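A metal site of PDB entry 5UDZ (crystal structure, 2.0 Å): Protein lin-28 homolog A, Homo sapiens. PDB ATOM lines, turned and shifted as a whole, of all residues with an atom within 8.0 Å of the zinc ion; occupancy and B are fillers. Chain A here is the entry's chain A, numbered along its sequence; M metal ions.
N of Cys 122 is in hydrogen-bond range of O of Ser 127, 2.8 Å away. N of Phe 124 sits close to SG of Cys 122 (3.3 Å). SG of Cys 135 lies close to N of Leu 137 (3.4 Å). The side-chain sulfur (SG) of Cys 135 lies close to the backbone NH (N) of Lys 138, 3.3 Å away. The side-chain sulfur (SG) of Cys 125 sits close to the backbone NH (N) of Ser 127. The backbone NH (N) of Ala 62 lies within hydrogen-bond range of the backbone carbonyl oxygen (O) of Cys 125.
Four residues have an atom within 4 Å of the zinc ion: Cys 122, Cys 125, His 130 and Cys 135.
The zinc ion is bound by a ring nitrogen (NE2) of His 130, the side-chain sulfur of Cys 122, the side-chain sulfur of Cys 135 and the side-chain sulfur of Cys 125.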
ATOM      1  N   LYS A  58      -7.888 -29.235 -35.879  1.00  0.00           N
ATOM      2  CA  LYS A  58      -6.550 -28.779 -36.231  1.00  0.00           C
ATOM      3  C   LYS A  58      -5.643 -28.866 -34.988  1.00  0.00           C
ATOM      4  O   LYS A  58      -6.100 -28.767 -33.836  1.00  0.00           O
ATOM      5  CB  LYS A  58      -6.564 -27.363 -36.776  1.00  0.00           C
ATOM      6  CG  LYS A  58      -6.959 -26.283 -35.768  1.00  0.00           C
ATOM      7  CD  LYS A  58      -6.943 -24.910 -36.425  1.00  0.00           C
ATOM      8  CE  LYS A  58      -6.883 -23.784 -35.402  1.00  0.00           C
ATOM      9  NZ  LYS A  58      -6.883 -22.453 -36.049  1.00  0.00           N
ATOM     10  N   GLY A  60      -3.401 -28.121 -32.082  1.00  0.00           N
ATOM     11  CA  GLY A  60      -3.352 -27.010 -31.157  1.00  0.00           C
ATOM     12  C   GLY A  60      -4.691 -26.476 -30.728  1.00  0.00           C
ATOM     13  O   GLY A  60      -4.721 -25.657 -29.814  1.00  0.00           O
ATOM     14  N   GLU A  61      -5.808 -26.905 -31.311  1.00  0.00           N
ATOM     15  CA  GLU A  61      -7.061 -26.296 -30.856  1.00  0.00           C
ATOM     16  C   GLU A  61      -7.473 -26.831 -29.503  1.00  0.00           C
ATOM     17  O   GLU A  61      -7.206 -27.984 -29.187  1.00  0.00           O
ATOM     18  CB  GLU A  61      -8.208 -26.423 -31.867  1.00  0.00           C
ATOM     19  CG  GLU A  61      -8.835 -27.762 -32.050  1.00  0.00           C
ATOM     20  CD  GLU A  61     -10.071 -27.650 -32.952  1.00  0.00           C
ATOM     21  OE1 GLU A  61      -9.930 -27.878 -34.173  1.00  0.00           O
ATOM     22  OE2 GLU A  61     -11.161 -27.319 -32.426  1.00  0.00           O
ATOM     23  N   ALA A  62      -8.086 -25.968 -28.689  1.00  0.00           N
ATOM     24  CA  ALA A  62      -8.451 -26.333 -27.328  1.00  0.00           C
ATOM     25  C   ALA A  62      -9.675 -27.236 -27.313  1.00  0.00           C
ATOM     26  O   ALA A  62     -10.633 -26.971 -28.028  1.00  0.00           O
ATOM     27  CB  ALA A  62      -8.743 -25.054 -26.532  1.00  0.00           C
ATOM     28  N   ILE A  88     -13.368 -26.444 -33.796  1.00  0.00           N
ATOM     29  CA  ILE A  88     -13.022 -25.495 -34.871  1.00  0.00           C
ATOM     30  C   ILE A  88     -12.798 -26.207 -36.183  1.00  0.00           C
ATOM     31  O   ILE A  88     -13.360 -25.859 -37.213  1.00  0.00           O
ATOM     32  CB  ILE A  88     -11.692 -24.750 -34.589  1.00  0.00           C
ATOM     33  CG1 ILE A  88     -11.798 -23.816 -33.387  1.00  0.00           C
ATOM     34  CG2 ILE A  88     -11.229 -23.946 -35.830  1.00  0.00           C
ATOM     35  CD1 ILE A  88     -10.465 -23.034 -33.073  1.00  0.00           C
ATOM     36  N   LYS A 121     -13.406 -17.243 -25.793  1.00  0.00           N
ATOM     37  CA  LYS A 121     -12.451 -18.164 -26.367  1.00  0.00           C
ATOM     38  C   LYS A 121     -11.604 -17.434 -27.390  1.00  0.00           C
ATOM     39  O   LYS A 121     -12.121 -16.604 -28.141  1.00  0.00           O
ATOM     40  CB  LYS A 121     -13.207 -19.305 -27.043  1.00  0.00           C
ATOM     41  CG  LYS A 121     -13.923 -20.243 -26.060  1.00  0.00           C
ATOM     42  CD  LYS A 121     -14.936 -21.157 -26.823  1.00  0.00           C
ATOM     43  CE  LYS A 121     -16.210 -20.359 -27.213  1.00  0.00           C
ATOM     44  NZ  LYS A 121     -16.942 -19.976 -25.971  1.00  0.00           N
ATOM     45  N   CYS A 122     -10.316 -17.774 -27.444  1.00  0.00           N
ATOM     46  CA  CYS A 122      -9.429 -17.250 -28.474  1.00  0.00           C
ATOM     47  C   CYS A 122     -10.045 -17.470 -29.840  1.00  0.00           C
ATOM     48  O   CYS A 122     -10.537 -18.570 -30.140  1.00  0.00           O
ATOM     49  CB  CYS A 122      -8.049 -17.923 -28.372  1.00  0.00           C
ATOM     50  SG  CYS A 122      -6.925 -17.525 -29.745  1.00  0.00           S
ATOM     51  N   HIS A 123     -10.056 -16.415 -30.649  1.00  0.00           N
ATOM     52  CA  HIS A 123     -10.619 -16.458 -31.995  1.00  0.00           C
ATOM     53  C   HIS A 123      -9.895 -17.450 -32.895  1.00  0.00           C
ATOM     54  O   HIS A 123     -10.457 -17.870 -33.876  1.00  0.00           O
ATOM     55  CB  HIS A 123     -10.561 -15.079 -32.676  1.00  0.00           C
ATOM     56  CG  HIS A 123     -11.486 -14.050 -32.090  1.00  0.00           C
ATOM     57  ND1 HIS A 123     -12.775 -14.341 -31.711  1.00  0.00           N
ATOM     58  CD2 HIS A 123     -11.304 -12.739 -31.834  1.00  0.00           C
ATOM     59  CE1 HIS A 123     -13.357 -13.242 -31.237  1.00  0.00           C
ATOM     60  NE2 HIS A 123     -12.466 -12.263 -31.274  1.00  0.00           N
ATOM     61  N   PHE A 124      -8.661 -17.804 -32.567  1.00  0.00           N
ATOM     62  CA  PHE A 124      -7.871 -18.660 -33.452  1.00  0.00           C
ATOM     63  C   PHE A 124      -7.772 -20.129 -32.966  1.00  0.00           C
ATOM     64  O   PHE A 124      -7.755 -21.040 -33.770  1.00  0.00           O
ATOM     65  CB  PHE A 124      -6.464 -18.076 -33.633  1.00  0.00           C
ATOM     66  CG  PHE A 124      -5.630 -18.799 -34.670  1.00  0.00           C
ATOM     67  CD1 PHE A 124      -5.814 -18.555 -36.018  1.00  0.00           C
ATOM     68  CD2 PHE A 124      -4.647 -19.707 -34.292  1.00  0.00           C
ATOM     69  CE1 PHE A 124      -5.049 -19.227 -36.977  1.00  0.00           C
ATOM     70  CE2 PHE A 124      -3.875 -20.359 -35.256  1.00  0.00           C
ATOM     71  CZ  PHE A 124      -4.079 -20.121 -36.584  1.00  0.00           C
ATOM     72  N   CYS A 125      -7.722 -20.352 -31.648  1.00  0.00           N
ATOM     73  CA  CYS A 125      -7.538 -21.721 -31.140  1.00  0.00           C
ATOM     74  C   CYS A 125      -8.572 -22.144 -30.071  1.00  0.00           C
ATOM     75  O   CYS A 125      -8.541 -23.259 -29.600  1.00  0.00           O
ATOM     76  CB  CYS A 125      -6.118 -21.872 -30.588  1.00  0.00           C
ATOM     77  SG  CYS A 125      -5.865 -21.177 -28.933  1.00  0.00           S
ATOM     78  N   GLN A 126      -9.496 -21.247 -29.729  1.00  0.00           N
ATOM     79  CA  GLN A 126     -10.547 -21.490 -28.737  1.00  0.00           C
ATOM     80  C   GLN A 126     -10.099 -21.629 -27.258  1.00  0.00           C
ATOM     81  O   GLN A 126     -10.936 -21.863 -26.372  1.00  0.00           O
ATOM     82  CB  GLN A 126     -11.501 -22.637 -29.170  1.00  0.00           C
ATOM     83  CG  GLN A 126     -12.539 -22.142 -30.203  1.00  0.00           C
ATOM     84  CD  GLN A 126     -13.886 -22.904 -30.213  1.00  0.00           C
ATOM     85  OE1 GLN A 126     -14.949 -22.285 -30.390  1.00  0.00           O
ATOM     86  NE2 GLN A 126     -13.835 -24.234 -30.110  1.00  0.00           N
ATOM     87  N   SER A 127      -8.819 -21.415 -26.974  1.00  0.00           N
ATOM     88  CA  SER A 127      -8.359 -21.374 -25.585  1.00  0.00           C
ATOM     89  C   SER A 127      -9.110 -20.326 -24.802  1.00  0.00           C
ATOM     90  O   SER A 127      -9.345 -19.246 -25.303  1.00  0.00           O
ATOM     91  CB  SER A 127      -6.877 -21.009 -25.487  1.00  0.00           C
ATOM     92  OG  SER A 127      -6.532 -20.891 -24.113  1.00  0.00           O
ATOM     93  N   ILE A 128      -9.438 -20.647 -23.547  1.00  0.00           N
ATOM     94  CA  ILE A 128     -10.065 -19.655 -22.669  1.00  0.00           C
ATOM     95  C   ILE A 128      -9.029 -18.961 -21.779  1.00  0.00           C
ATOM     96  O   ILE A 128      -9.392 -18.175 -20.913  1.00  0.00           O
ATOM     97  CB  ILE A 128     -11.182 -20.273 -21.792  1.00  0.00           C
ATOM     98  CG1 ILE A 128     -10.636 -21.385 -20.913  1.00  0.00           C
ATOM     99  CG2 ILE A 128     -12.328 -20.796 -22.666  1.00  0.00           C
ATOM    100  CD1 ILE A 128     -11.603 -21.851 -19.813  1.00  0.00           C
ATOM    101  N   SER A 129      -7.750 -19.232 -21.990  1.00  0.00           N
ATOM    102  CA  SER A 129      -6.730 -18.622 -21.147  1.00  0.00           C
ATOM    103  C   SER A 129      -5.970 -17.461 -21.830  1.00  0.00           C
ATOM    104  O   SER A 129      -5.176 -16.783 -21.192  1.00  0.00           O
ATOM    105  CB  SER A 129      -5.753 -19.667 -20.591  1.00  0.00           C
ATOM    106  OG  SER A 129      -5.149 -20.437 -21.606  1.00  0.00           O
ATOM    107  N   HIS A 130      -6.241 -17.246 -23.114  1.00  0.00           N
ATOM    108  CA  HIS A 130      -5.734 -16.066 -23.804  1.00  0.00           C
ATOM    109  C   HIS A 130      -6.708 -15.670 -24.898  1.00  0.00           C
ATOM    110  O   HIS A 130      -7.561 -16.458 -25.310  1.00  0.00           O
ATOM    111  CB  HIS A 130      -4.362 -16.326 -24.414  1.00  0.00           C
ATOM    112  CG  HIS A 130      -4.381 -17.351 -25.504  1.00  0.00           C
ATOM    113  ND1 HIS A 130      -4.002 -18.660 -25.305  1.00  0.00           N
ATOM    114  CD2 HIS A 130      -4.738 -17.257 -26.818  1.00  0.00           C
ATOM    115  CE1 HIS A 130      -4.128 -19.327 -26.437  1.00  0.00           C
ATOM    116  NE2 HIS A 130      -4.582 -18.509 -27.358  1.00  0.00           N
ATOM    117  N   MET A 131      -6.581 -14.426 -25.334  1.00  0.00           N
ATOM    118  CA  MET A 131      -7.268 -13.908 -26.495  1.00  0.00           C
ATOM    119  C   MET A 131      -6.273 -13.834 -27.662  1.00  0.00           C
ATOM    120  O   MET A 131      -5.073 -14.001 -27.492  1.00  0.00           O
ATOM    121  CB  MET A 131      -7.859 -12.546 -26.167  1.00  0.00           C
ATOM    122  CG  MET A 131      -9.101 -12.642 -25.212  1.00  0.00           C
ATOM    123  SD  MET A 131      -9.819 -11.038 -24.845  1.00  0.00           S
ATOM    124  CE  MET A 131      -8.489 -10.199 -23.994  1.00  0.00           C
ATOM    125  N   VAL A 132      -6.796 -13.602 -28.860  1.00  0.00           N
ATOM    126  CA  VAL A 132      -6.058 -13.915 -30.070  1.00  0.00           C
ATOM    127  C   VAL A 132      -4.807 -13.050 -30.217  1.00  0.00           C
ATOM    128  O   VAL A 132      -3.813 -13.492 -30.789  1.00  0.00           O
ATOM    129  CB  VAL A 132      -6.955 -13.790 -31.345  1.00  0.00           C
ATOM    130  CG1 VAL A 132      -7.319 -12.332 -31.614  1.00  0.00           C
ATOM    131  CG2 VAL A 132      -6.250 -14.379 -32.545  1.00  0.00           C
ATOM    132  N   ALA A 133      -4.825 -11.829 -29.661  1.00  0.00           N
ATOM    133  CA  ALA A 133      -3.637 -10.956 -29.756  1.00  0.00           C
ATOM    134  C   ALA A 133      -2.434 -11.585 -29.070  1.00  0.00           C
ATOM    135  O   ALA A 133      -1.307 -11.189 -29.344  1.00  0.00           O
ATOM    136  CB  ALA A 133      -3.897  -9.552 -29.187  1.00  0.00           C
ATOM    137  N   SER A 134      -2.657 -12.568 -28.200  1.00  0.00           N
ATOM    138  CA  SER A 134      -1.551 -13.265 -27.546  1.00  0.00           C
ATOM    139  C   SER A 134      -1.526 -14.764 -27.897  1.00  0.00           C
ATOM    140  O   SER A 134      -0.916 -15.563 -27.188  1.00  0.00           O
ATOM    141  CB  SER A 134      -1.647 -13.124 -26.041  1.00  0.00           C
ATOM    142  OG  SER A 134      -1.548 -11.748 -25.650  1.00  0.00           O
ATOM    143  N   CYS A 135      -2.151 -15.154 -28.999  1.00  0.00           N
ATOM    144  CA  CYS A 135      -2.233 -16.604 -29.322  1.00  0.00           C
ATOM    145  C   CYS A 135      -0.895 -17.202 -29.772  1.00  0.00           C
ATOM    146  O   CYS A 135      -0.337 -16.765 -30.782  1.00  0.00           O
ATOM    147  CB  CYS A 135      -3.310 -16.848 -30.336  1.00  0.00           C
ATOM    148  SG  CYS A 135      -3.418 -18.594 -30.762  1.00  0.00           S
ATOM    149  N   PRO A 136      -0.351 -18.178 -29.008  1.00  0.00           N
ATOM    150  CA  PRO A 136       0.951 -18.690 -29.490  1.00  0.00           C
ATOM    151  C   PRO A 136       0.791 -19.588 -30.692  1.00  0.00           C
ATOM    152  O   PRO A 136       1.738 -19.721 -31.466  1.00  0.00           O
ATOM    153  CB  PRO A 136       1.496 -19.492 -28.289  1.00  0.00           C
ATOM    154  CG  PRO A 136       0.304 -19.891 -27.522  1.00  0.00           C
ATOM    155  CD  PRO A 136      -0.722 -18.788 -27.715  1.00  0.00           C
ATOM    156  N   LEU A 137      -0.394 -20.170 -30.874  1.00  0.00           N
ATOM    157  CA  LEU A 137      -0.607 -21.043 -32.020  1.00  0.00           C
ATOM    158  C   LEU A 137      -0.573 -20.188 -33.259  1.00  0.00           C
ATOM    159  O   LEU A 137       0.081 -20.535 -34.217  1.00  0.00           O
ATOM    160  CB  LEU A 137      -1.971 -21.754 -31.970  1.00  0.00           C
ATOM    161  CG  LEU A 137      -2.204 -22.897 -32.979  1.00  0.00           C
ATOM    162  CD1 LEU A 137      -1.161 -24.004 -32.758  1.00  0.00           C
ATOM    163  CD2 LEU A 137      -3.649 -23.455 -32.859  1.00  0.00           C
ATOM    164  N   LYS A 138      -1.276 -19.068 -33.240  1.00  0.00           N
ATOM    165  CA  LYS A 138      -1.271 -18.194 -34.406  1.00  0.00           C
ATOM    166  C   LYS A 138       0.146 -17.686 -34.719  1.00  0.00           C
ATOM    167  O   LYS A 138       0.540 -17.599 -35.877  1.00  0.00           O
ATOM    168  CB  LYS A 138      -2.199 -17.026 -34.209  1.00  0.00           C
ATOM    169  CG  LYS A 138      -2.411 -16.259 -35.458  1.00  0.00           C
ATOM    170  CD  LYS A 138      -3.524 -15.252 -35.292  1.00  0.00           C
ATOM    171  CE  LYS A 138      -3.580 -14.329 -36.478  1.00  0.00           C
ATOM    172  NZ  LYS A 138      -4.663 -13.365 -36.255  1.00  0.00           N
ATOM    173  N   ALA A 139       0.916 -17.392 -33.675  1.00  0.00           N
ATOM    174  CA  ALA A 139       2.291 -16.893 -33.827  1.00  0.00           C
ATOM    175  C   ALA A 139       3.252 -17.897 -34.493  1.00  0.00           C
ATOM    176  O   ALA A 139       4.136 -17.494 -35.234  1.00  0.00           O
ATOM    177  CB  ALA A 139       2.846 -16.472 -32.485  1.00  0.00           C
HETATM  178 ZN    ZN M   1      -5.154 -18.948 -29.254  1.00  0.00          ZN
